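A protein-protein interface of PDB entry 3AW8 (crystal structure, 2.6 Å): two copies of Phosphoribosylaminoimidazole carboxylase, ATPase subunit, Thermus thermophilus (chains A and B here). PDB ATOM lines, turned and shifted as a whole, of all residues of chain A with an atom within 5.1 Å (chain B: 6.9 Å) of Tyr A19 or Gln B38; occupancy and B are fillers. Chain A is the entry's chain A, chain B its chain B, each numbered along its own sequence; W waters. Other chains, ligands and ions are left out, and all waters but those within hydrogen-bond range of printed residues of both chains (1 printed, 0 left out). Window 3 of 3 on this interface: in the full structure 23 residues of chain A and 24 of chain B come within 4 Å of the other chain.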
ATOM      1  N   ALA A  15      -3.110  26.509  -0.095  1.00  0.00           N
ATOM      2  CA  ALA A  15      -2.183  26.263   1.001  1.00  0.00           C
ATOM      3  C   ALA A  15      -2.835  25.476   2.143  1.00  0.00           C
ATOM      4  O   ALA A  15      -2.238  24.527   2.661  1.00  0.00           O
ATOM      5  CB  ALA A  15      -1.606  27.588   1.517  1.00  0.00           C
ATOM      6  N   LEU A  16      -4.050  25.860   2.536  1.00  0.00           N
ATOM      7  CA  LEU A  16      -4.744  25.155   3.626  1.00  0.00           C
ATOM      8  C   LEU A  16      -4.986  23.705   3.253  1.00  0.00           C
ATOM      9  O   LEU A  16      -4.927  22.825   4.107  1.00  0.00           O
ATOM     10  CB  LEU A  16      -6.078  25.830   3.966  1.00  0.00           C
ATOM     11  CG  LEU A  16      -5.934  27.251   4.545  1.00  0.00           C
ATOM     12  CD1 LEU A  16      -7.310  27.898   4.713  1.00  0.00           C
ATOM     13  CD2 LEU A  16      -5.200  27.194   5.869  1.00  0.00           C
ATOM     14  N   ALA A  17      -5.244  23.449   1.974  1.00  0.00           N
ATOM     15  CA  ALA A  17      -5.468  22.078   1.537  1.00  0.00           C
ATOM     16  C   ALA A  17      -4.139  21.315   1.429  1.00  0.00           C
ATOM     17  O   ALA A  17      -4.115  20.089   1.504  1.00  0.00           O
ATOM     18  CB  ALA A  17      -6.209  22.067   0.188  1.00  0.00           C
ATOM     19  N   GLY A  18      -3.036  22.043   1.279  1.00  0.00           N
ATOM     20  CA  GLY A  18      -1.738  21.405   1.135  1.00  0.00           C
ATOM     21  C   GLY A  18      -0.973  21.062   2.398  1.00  0.00           C
ATOM     22  O   GLY A  18      -0.198  20.097   2.414  1.00  0.00           O
ATOM     23  N   TYR A  19      -1.153  21.839   3.460  1.00  0.00           N
ATOM     24  CA  TYR A  19      -0.432  21.549   4.697  1.00  0.00           C
ATOM     25  C   TYR A  19      -0.690  20.124   5.220  1.00  0.00           C
ATOM     26  O   TYR A  19       0.212  19.486   5.757  1.00  0.00           O
ATOM     27  CB  TYR A  19      -0.779  22.585   5.767  1.00  0.00           C
ATOM     28  CG  TYR A  19      -0.112  23.918   5.549  1.00  0.00           C
ATOM     29  CD1 TYR A  19       1.283  24.030   5.553  1.00  0.00           C
ATOM     30  CD2 TYR A  19      -0.864  25.072   5.323  1.00  0.00           C
ATOM     31  CE1 TYR A  19       1.916  25.250   5.336  1.00  0.00           C
ATOM     32  CE2 TYR A  19      -0.241  26.303   5.104  1.00  0.00           C
ATOM     33  CZ  TYR A  19       1.151  26.381   5.114  1.00  0.00           C
ATOM     34  OH  TYR A  19       1.772  27.587   4.909  1.00  0.00           O
ATOM     35  N   PRO A  20      -1.923  19.607   5.080  1.00  0.00           N
ATOM     36  CA  PRO A  20      -2.153  18.247   5.578  1.00  0.00           C
ATOM     37  C   PRO A  20      -1.300  17.234   4.825  1.00  0.00           C
ATOM     38  O   PRO A  20      -1.073  16.126   5.313  1.00  0.00           O
ATOM     39  CB  PRO A  20      -3.645  18.035   5.343  1.00  0.00           C
ATOM     40  CG  PRO A  20      -4.193  19.422   5.472  1.00  0.00           C
ATOM     41  CD  PRO A  20      -3.193  20.247   4.702  1.00  0.00           C
ATOM     42  N   LEU A  21      -0.835  17.610   3.634  1.00  0.00           N
ATOM     43  CA  LEU A  21       0.009  16.730   2.832  1.00  0.00           C
ATOM     44  C   LEU A  21       1.473  17.044   3.112  1.00  0.00           C
ATOM     45  O   LEU A  21       2.361  16.594   2.397  1.00  0.00           O
ATOM     46  CB  LEU A  21      -0.277  16.908   1.335  1.00  0.00           C
ATOM     47  CG  LEU A  21      -1.647  16.444   0.828  1.00  0.00           C
ATOM     48  CD1 LEU A  21      -1.833  16.869  -0.602  1.00  0.00           C
ATOM     49  CD2 LEU A  21      -1.762  14.939   0.933  1.00  0.00           C
ATOM     50  N   GLY A  22       1.710  17.834   4.153  1.00  0.00           N
ATOM     51  CA  GLY A  22       3.065  18.196   4.523  1.00  0.00           C
ATOM     52  C   GLY A  22       3.813  19.086   3.549  1.00  0.00           C
ATOM     53  O   GLY A  22       5.046  19.112   3.562  1.00  0.00           O
ATOM     54  N   LEU A  23       3.084  19.816   2.711  1.00  0.00           N
ATOM     55  CA  LEU A  23       3.697  20.707   1.735  1.00  0.00           C
ATOM     56  C   LEU A  23       4.020  22.095   2.313  1.00  0.00           C
ATOM     57  O   LEU A  23       3.652  22.422   3.445  1.00  0.00           O
ATOM     58  CB  LEU A  23       2.775  20.867   0.528  1.00  0.00           C
ATOM     59  CG  LEU A  23       2.287  19.595  -0.180  1.00  0.00           C
ATOM     60  CD1 LEU A  23       1.255  19.958  -1.240  1.00  0.00           C
ATOM     61  CD2 LEU A  23       3.470  18.863  -0.814  1.00  0.00           C
ATOM     62  N   SER A  24       4.714  22.902   1.518  1.00  0.00           N
ATOM     63  CA  SER A  24       5.097  24.260   1.902  1.00  0.00           C
ATOM     64  C   SER A  24       4.694  25.200   0.786  1.00  0.00           C
ATOM     65  O   SER A  24       4.598  24.797  -0.375  1.00  0.00           O
ATOM     66  CB  SER A  24       6.598  24.356   2.119  1.00  0.00           C
ATOM     67  OG  SER A  24       6.970  23.503   3.172  1.00  0.00           O
ATOM     68  N   PHE A  25       4.482  26.461   1.123  1.00  0.00           N
ATOM     69  CA  PHE A  25       4.041  27.410   0.118  1.00  0.00           C
ATOM     70  C   PHE A  25       4.712  28.752   0.223  1.00  0.00           C
ATOM     71  O   PHE A  25       5.190  29.131   1.290  1.00  0.00           O
ATOM     72  CB  PHE A  25       2.518  27.600   0.236  1.00  0.00           C
ATOM     73  CG  PHE A  25       1.744  26.343   0.018  1.00  0.00           C
ATOM     74  CD1 PHE A  25       1.307  25.994  -1.251  1.00  0.00           C
ATOM     75  CD2 PHE A  25       1.520  25.464   1.072  1.00  0.00           C
ATOM     76  CE1 PHE A  25       0.654  24.778  -1.476  1.00  0.00           C
ATOM     77  CE2 PHE A  25       0.872  24.246   0.864  1.00  0.00           C
ATOM     78  CZ  PHE A  25       0.437  23.900  -0.414  1.00  0.00           C
ATOM     79  N   VAL A  39      -1.396  32.921   5.807  1.00  0.00           N
ATOM     80  CA  VAL A  39      -1.332  31.478   5.865  1.00  0.00           C
ATOM     81  C   VAL A  39      -0.042  30.857   5.342  1.00  0.00           C
ATOM     82  O   VAL A  39       0.187  29.661   5.513  1.00  0.00           O
ATOM     83  CB  VAL A  39      -2.578  30.933   5.123  1.00  0.00           C
ATOM     84  CG1 VAL A  39      -2.180  30.177   3.872  1.00  0.00           C
ATOM     85  CG2 VAL A  39      -3.427  30.133   6.073  1.00  0.00           C
ATOM     86  N   GLY A  40       0.805  31.668   4.719  1.00  0.00           N
ATOM     87  CA  GLY A  40       2.069  31.169   4.202  1.00  0.00           C
ATOM     88  C   GLY A  40       3.062  32.295   3.986  1.00  0.00           C
ATOM     89  O   GLY A  40       2.799  33.431   4.372  1.00  0.00           O
ATOM     90  N   GLY B   7       3.399  23.747  20.431  1.00  0.00           N
ATOM     91  CA  GLY B   7       3.467  23.926  18.992  1.00  0.00           C
ATOM     92  C   GLY B   7       3.390  22.630  18.211  1.00  0.00           C
ATOM     93  O   GLY B   7       3.758  22.589  17.029  1.00  0.00           O
ATOM     94  N   ARG B  12      -1.171  22.554  15.398  1.00  0.00           N
ATOM     95  CA  ARG B  12      -1.124  22.768  13.957  1.00  0.00           C
ATOM     96  C   ARG B  12      -2.493  22.519  13.341  1.00  0.00           C
ATOM     97  O   ARG B  12      -2.940  23.274  12.491  1.00  0.00           O
ATOM     98  CB  ARG B  12      -0.085  21.838  13.334  1.00  0.00           C
ATOM     99  CG  ARG B  12      -0.047  21.811  11.824  1.00  0.00           C
ATOM    100  CD  ARG B  12       0.938  20.739  11.410  1.00  0.00           C
ATOM    101  NE  ARG B  12       0.914  20.427   9.990  1.00  0.00           N
ATOM    102  CZ  ARG B  12       1.793  20.884   9.107  1.00  0.00           C
ATOM    103  NH1 ARG B  12       2.775  21.689   9.495  1.00  0.00           N
ATOM    104  NH2 ARG B  12       1.702  20.516   7.836  1.00  0.00           N
ATOM    105  N   LEU B  16      -5.264  25.131  11.406  1.00  0.00           N
ATOM    106  CA  LEU B  16      -5.833  24.780  10.093  1.00  0.00           C
ATOM    107  C   LEU B  16      -7.352  24.816  10.114  1.00  0.00           C
ATOM    108  O   LEU B  16      -7.974  25.220   9.143  1.00  0.00           O
ATOM    109  CB  LEU B  16      -5.374  23.386   9.643  1.00  0.00           C
ATOM    110  CG  LEU B  16      -4.144  23.235   8.726  1.00  0.00           C
ATOM    111  CD1 LEU B  16      -3.440  24.561   8.477  1.00  0.00           C
ATOM    112  CD2 LEU B  16      -3.202  22.231   9.351  1.00  0.00           C
ATOM    113  N   TYR B  19      -8.271  28.928  10.418  1.00  0.00           N
ATOM    114  CA  TYR B  19      -8.143  29.898   9.336  1.00  0.00           C
ATOM    115  C   TYR B  19      -9.447  30.064   8.543  1.00  0.00           C
ATOM    116  O   TYR B  19      -9.813  31.175   8.179  1.00  0.00           O
ATOM    117  CB  TYR B  19      -6.979  29.524   8.413  1.00  0.00           C
ATOM    118  CG  TYR B  19      -5.637  29.833   9.026  1.00  0.00           C
ATOM    119  CD1 TYR B  19      -5.296  31.146   9.375  1.00  0.00           C
ATOM    120  CD2 TYR B  19      -4.735  28.812   9.333  1.00  0.00           C
ATOM    121  CE1 TYR B  19      -4.101  31.435  10.025  1.00  0.00           C
ATOM    122  CE2 TYR B  19      -3.535  29.091   9.986  1.00  0.00           C
ATOM    123  CZ  TYR B  19      -3.230  30.406  10.330  1.00  0.00           C
ATOM    124  OH  TYR B  19      -2.062  30.683  10.997  1.00  0.00           O
ATOM    125  N   PHE B  27       1.642  30.455  18.591  1.00  0.00           N
ATOM    126  CA  PHE B  27       1.987  29.281  19.377  1.00  0.00           C
ATOM    127  C   PHE B  27       3.187  29.586  20.231  1.00  0.00           C
ATOM    128  O   PHE B  27       3.983  30.465  19.898  1.00  0.00           O
ATOM    129  CB  PHE B  27       2.325  28.083  18.472  1.00  0.00           C
ATOM    130  CG  PHE B  27       1.215  27.686  17.542  1.00  0.00           C
ATOM    131  CD1 PHE B  27       1.108  28.263  16.280  1.00  0.00           C
ATOM    132  CD2 PHE B  27       0.255  26.760  17.943  1.00  0.00           C
ATOM    133  CE1 PHE B  27       0.054  27.923  15.423  1.00  0.00           C
ATOM    134  CE2 PHE B  27      -0.793  26.415  17.100  1.00  0.00           C
ATOM    135  CZ  PHE B  27      -0.892  27.003  15.831  1.00  0.00           C
ATOM    136  N   GLU B  33      11.460  23.973  16.011  1.00  0.00           N
ATOM    137  CA  GLU B  33      10.925  23.134  14.946  1.00  0.00           C
ATOM    138  C   GLU B  33       9.464  22.749  15.095  1.00  0.00           C
ATOM    139  O   GLU B  33       8.948  22.030  14.250  1.00  0.00           O
ATOM    140  CB  GLU B  33      11.754  21.854  14.819  1.00  0.00           C
ATOM    141  CG  GLU B  33      13.244  22.101  14.756  1.00  0.00           C
ATOM    142  CD  GLU B  33      13.619  23.058  13.637  1.00  0.00           C
ATOM    143  OE1 GLU B  33      14.749  23.600  13.667  1.00  0.00           O
ATOM    144  OE2 GLU B  33      12.786  23.264  12.724  1.00  0.00           O
ATOM    145  N   ALA B  34       8.806  23.208  16.157  1.00  0.00           N
ATOM    146  CA  ALA B  34       7.390  22.880  16.381  1.00  0.00           C
ATOM    147  C   ALA B  34       6.657  22.909  15.041  1.00  0.00           C
ATOM    148  O   ALA B  34       6.645  23.924  14.353  1.00  0.00           O
ATOM    149  CB  ALA B  34       6.762  23.877  17.352  1.00  0.00           C
ATOM    150  N   CYS B  35       6.045  21.796  14.665  1.00  0.00           N
ATOM    151  CA  CYS B  35       5.382  21.761  13.375  1.00  0.00           C
ATOM    152  C   CYS B  35       4.265  22.795  13.230  1.00  0.00           C
ATOM    153  O   CYS B  35       3.894  23.154  12.103  1.00  0.00           O
ATOM    154  CB  CYS B  35       4.869  20.345  13.062  1.00  0.00           C
ATOM    155  SG  CYS B  35       3.598  19.730  14.142  1.00  0.00           S
ATOM    156  N   ALA B  36       3.738  23.293  14.349  1.00  0.00           N
ATOM    157  CA  ALA B  36       2.683  24.295  14.256  1.00  0.00           C
ATOM    158  C   ALA B  36       3.286  25.570  13.677  1.00  0.00           C
ATOM    159  O   ALA B  36       2.590  26.378  13.053  1.00  0.00           O
ATOM    160  CB  ALA B  36       2.080  24.572  15.610  1.00  0.00           C
ATOM    161  N   GLY B  37       4.591  25.733  13.876  1.00  0.00           N
ATOM    162  CA  GLY B  37       5.275  26.903  13.366  1.00  0.00           C
ATOM    163  C   GLY B  37       5.136  27.048  11.863  1.00  0.00           C
ATOM    164  O   GLY B  37       5.279  28.144  11.321  1.00  0.00           O
ATOM    165  N   GLN B  38       4.855  25.949  11.180  1.00  0.00           N
ATOM    166  CA  GLN B  38       4.708  25.983   9.734  1.00  0.00           C
ATOM    167  C   GLN B  38       3.366  26.568   9.300  1.00  0.00           C
ATOM    168  O   GLN B  38       3.152  26.822   8.114  1.00  0.00           O
ATOM    169  CB  GLN B  38       4.860  24.568   9.164  1.00  0.00           C
ATOM    170  CG  GLN B  38       6.269  23.988   9.273  1.00  0.00           C
ATOM    171  CD  GLN B  38       6.289  22.461   9.286  1.00  0.00           C
ATOM    172  OE1 GLN B  38       5.439  21.807   8.678  1.00  0.00           O
ATOM    173  NE2 GLN B  38       7.277  21.890   9.976  1.00  0.00           N
ATOM    174  N   VAL B  39       2.462  26.798  10.247  1.00  0.00           N
ATOM    175  CA  VAL B  39       1.154  27.325   9.883  1.00  0.00           C
ATOM    176  C   VAL B  39       0.707  28.564  10.656  1.00  0.00           C
ATOM    177  O   VAL B  39      -0.380  29.087  10.416  1.00  0.00           O
ATOM    178  CB  VAL B  39       0.061  26.225  10.002  1.00  0.00           C
ATOM    179  CG1 VAL B  39       0.422  25.045   9.117  1.00  0.00           C
ATOM    180  CG2 VAL B  39      -0.094  25.789  11.446  1.00  0.00           C
ATOM    181  N   GLY B  40       1.543  29.049  11.565  1.00  0.00           N
ATOM    182  CA  GLY B  40       1.181  30.238  12.322  1.00  0.00           C
ATOM    183  C   GLY B  40       2.424  30.837  12.927  1.00  0.00           C
ATOM    184  O   GLY B  40       3.498  30.270  12.746  1.00  0.00           O
ATOM    185  N   LEU B  42       5.051  31.304  15.561  1.00  0.00           N
ATOM    186  CA  LEU B  42       5.517  30.515  16.673  1.00  0.00           C
ATOM    187  C   LEU B  42       6.556  31.267  17.478  1.00  0.00           C
ATOM    188  O   LEU B  42       7.556  31.736  16.944  1.00  0.00           O
ATOM    189  CB  LEU B  42       6.096  29.204  16.126  1.00  0.00           C
ATOM    190  CG  LEU B  42       6.808  28.188  17.016  1.00  0.00           C
ATOM    191  CD1 LEU B  42       8.285  28.482  17.035  1.00  0.00           C
ATOM    192  CD2 LEU B  42       6.197  28.194  18.407  1.00  0.00           C
ATOM    193  N   LEU B 323      -4.713  11.601   3.694  1.00  0.00           N
ATOM    194  CA  LEU B 323      -3.395  11.685   4.305  1.00  0.00           C
ATOM    195  C   LEU B 323      -3.182  12.986   5.089  1.00  0.00           C
ATOM    196  O   LEU B 323      -3.634  14.062   4.675  1.00  0.00           O
ATOM    197  CB  LEU B 323      -2.316  11.558   3.229  1.00  0.00           C
ATOM    198  CG  LEU B 323      -0.891  11.610   3.771  1.00  0.00           C
ATOM    199  CD1 LEU B 323      -0.668  10.382   4.642  1.00  0.00           C
ATOM    200  CD2 LEU B 323       0.132  11.680   2.626  1.00  0.00           C
ATOM    201  N   HIS B 324      -2.489  12.871   6.218  1.00  0.00           N
ATOM    202  CA  HIS B 324      -2.184  14.022   7.071  1.00  0.00           C
ATOM    203  C   HIS B 324      -0.757  13.896   7.570  1.00  0.00           C
ATOM    204  O   HIS B 324      -0.488  13.152   8.503  1.00  0.00           O
ATOM    205  CB  HIS B 324      -3.139  14.070   8.260  1.00  0.00           C
ATOM    206  CG  HIS B 324      -4.515  14.530   7.904  1.00  0.00           C
ATOM    207  ND1 HIS B 324      -4.882  15.859   7.915  1.00  0.00           N
ATOM    208  CD2 HIS B 324      -5.598  13.844   7.470  1.00  0.00           C
ATOM    209  CE1 HIS B 324      -6.130  15.973   7.500  1.00  0.00           C
ATOM    210  NE2 HIS B 324      -6.588  14.765   7.222  1.00  0.00           N
ATOM    211  N   TRP B 325       0.163  14.604   6.932  1.00  0.00           N
ATOM    212  CA  TRP B 325       1.559  14.563   7.330  1.00  0.00           C
ATOM    213  C   TRP B 325       1.790  15.808   8.183  1.00  0.00           C
ATOM    214  O   TRP B 325       1.511  16.922   7.744  1.00  0.00           O
ATOM    215  CB  TRP B 325       2.450  14.562   6.084  1.00  0.00           C
ATOM    216  CG  TRP B 325       3.873  14.268   6.394  1.00  0.00           C
ATOM    217  CD1 TRP B 325       4.932  15.110   6.243  1.00  0.00           C
ATOM    218  CD2 TRP B 325       4.390  13.069   6.980  1.00  0.00           C
ATOM    219  NE1 TRP B 325       6.079  14.514   6.704  1.00  0.00           N
ATOM    220  CE2 TRP B 325       5.776  13.260   7.163  1.00  0.00           C
ATOM    221  CE3 TRP B 325       3.814  11.852   7.377  1.00  0.00           C
ATOM    222  CZ2 TRP B 325       6.600  12.283   7.723  1.00  0.00           C
ATOM    223  CZ3 TRP B 325       4.637  10.876   7.942  1.00  0.00           C
ATOM    224  CH2 TRP B 325       6.014  11.103   8.108  1.00  0.00           C
ATOM    225  N   TYR B 326       2.300  15.632   9.398  1.00  0.00           N
ATOM    226  CA  TYR B 326       2.480  16.774  10.295  1.00  0.00           C
ATOM    227  C   TYR B 326       3.635  17.727  10.039  1.00  0.00           C
ATOM    228  O   TYR B 326       3.645  18.822  10.586  1.00  0.00           O
ATOM    229  CB  TYR B 326       2.531  16.297  11.748  1.00  0.00           C
ATOM    230  CG  TYR B 326       1.372  15.400  12.133  1.00  0.00           C
ATOM    231  CD1 TYR B 326       0.107  15.577  11.564  1.00  0.00           C
ATOM    232  CD2 TYR B 326       1.536  14.384  13.080  1.00  0.00           C
ATOM    233  CE1 TYR B 326      -0.957  14.774  11.922  1.00  0.00           C
ATOM    234  CE2 TYR B 326       0.474  13.574  13.448  1.00  0.00           C
ATOM    235  CZ  TYR B 326      -0.774  13.779  12.864  1.00  0.00           C
ATOM    236  OH  TYR B 326      -1.849  13.011  13.246  1.00  0.00           O
ATOM    237  N   GLY B 327       4.599  17.323   9.215  1.00  0.00           N
ATOM    238  CA  GLY B 327       5.734  18.184   8.929  1.00  0.00           C
ATOM    239  C   GLY B 327       6.880  17.992   9.901  1.00  0.00           C
ATOM    240  O   GLY B 327       7.858  18.729   9.882  1.00  0.00           O
ATOM    241  N   LYS B 328       6.772  16.997  10.765  1.00  0.00           N
ATOM    242  CA  LYS B 328       7.829  16.746  11.727  1.00  0.00           C
ATOM    243  C   LYS B 328       8.877  15.828  11.119  1.00  0.00           C
ATOM    244  O   LYS B 328       8.612  15.128  10.145  1.00  0.00           O
ATOM    245  CB  LYS B 328       7.251  16.116  13.000  1.00  0.00           C
ATOM    246  CG  LYS B 328       6.061  16.893  13.560  1.00  0.00           C
ATOM    247  CD  LYS B 328       5.888  16.678  15.057  1.00  0.00           C
ATOM    248  CE  LYS B 328       5.136  15.419  15.386  1.00  0.00           C
ATOM    249  NZ  LYS B 328       5.158  15.121  16.843  1.00  0.00           N
ATOM    250  N   ALA B 329      10.078  15.861  11.683  1.00  0.00           N
ATOM    251  CA  ALA B 329      11.167  15.014  11.224  1.00  0.00           C
ATOM    252  C   ALA B 329      10.844  13.614  11.711  1.00  0.00           C
ATOM    253  O   ALA B 329      10.443  13.440  12.860  1.00  0.00           O
ATOM    254  CB  ALA B 329      12.477  15.482  11.827  1.00  0.00           C
HETATM  255  O   HOH W   1      -0.892  18.289   8.812  1.00  0.00           O
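NH2 of Arg B12 sits at hydrogen-bond distance from O of Tyr A19 (2.8 Å). The backbone carbonyl oxygen of Pro A20 lies within hydrogen-bond range of the backbone NH of Trp B325 (2.5 Å). The backbone carbonyl oxygen of Tyr A19 sits close to the backbone carbonyl oxygen of Trp B325 (3.5 Å). The backbone carbonyl oxygen (O) of Leu B323 lies close to the backbone carbonyl oxygen (O) of Pro A20.
The backbone carbonyl oxygen (O) of Val A39 is in hydrogen-bond range of the side-chain hydroxyl (OH) of Tyr A19. The backbone carbonyl oxygen (O) of Cys B35 is in hydrogen-bond range of the guanidinium group (NH1) of Arg B12. The side-chain amide oxygen of Gln B38 sits at hydrogen-bond distance from the guanidinium group of Arg B12, 2.8 Å away. NH1 of Arg B12 sits close to O of Tyr B326 (3.2 Å). The side-chain amide nitrogen of Gln B38 lies within hydrogen-bond range of the backbone carbonyl oxygen of Gly B327 (3.2 Å).
Among the printed residues, merely in contact across the chains: Leu A16 with Tyr B19 (3.9 Å), Tyr A19 with Gln B38 (3.4 Å), Tyr A19 with Val B39 (3.8 Å), Pro A20 with His B324 (3.0 Å), Leu A21 with Trp B325 (3.99 Å), Gly A22 with Trp B325 (3.7 Å) and Val A39 with Tyr B19 (3.7 Å).
Tyr A19 touches four residues of chain B. Of the printed residues of chain A, Arg B12 touches Tyr A19. Printed residues of chain A within 4 Å of Leu B323: Pro A20 (3.4 Å). Of the printed residues of chain A, Trp B325 touches Tyr A19, Pro A20, Leu A21 and Gly A22. The nearest residue of chain B that does not touch Tyr A19 is Leu B16 (4.1 Å).
Printed residues of chain A that touch a printed residue of chain B: Leu A16, Tyr A19, Pro A20, Leu A21, Gly A22 and Val A39. Of the 21 printed residues of chain B, 7 touch a printed residue of chain A. Among the printed residues, 11 pairs touch across the chains. Among the printed residues, no Asp or Glu carboxylate lies within 4 Å of a Lys or Arg side-chain nitrogen of the other chain.
Leu A16 touches Tyr B19, but with the chains exchanged Tyr A19 does not touch Leu B16 (4.1 Å). Tyr A19 touches Val B39, and with the chains exchanged Val A39 touches Tyr B19.
Water W1 lies within hydrogen-bond range of O of Trp B325, NE of Arg B12 and O of Tyr A19.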
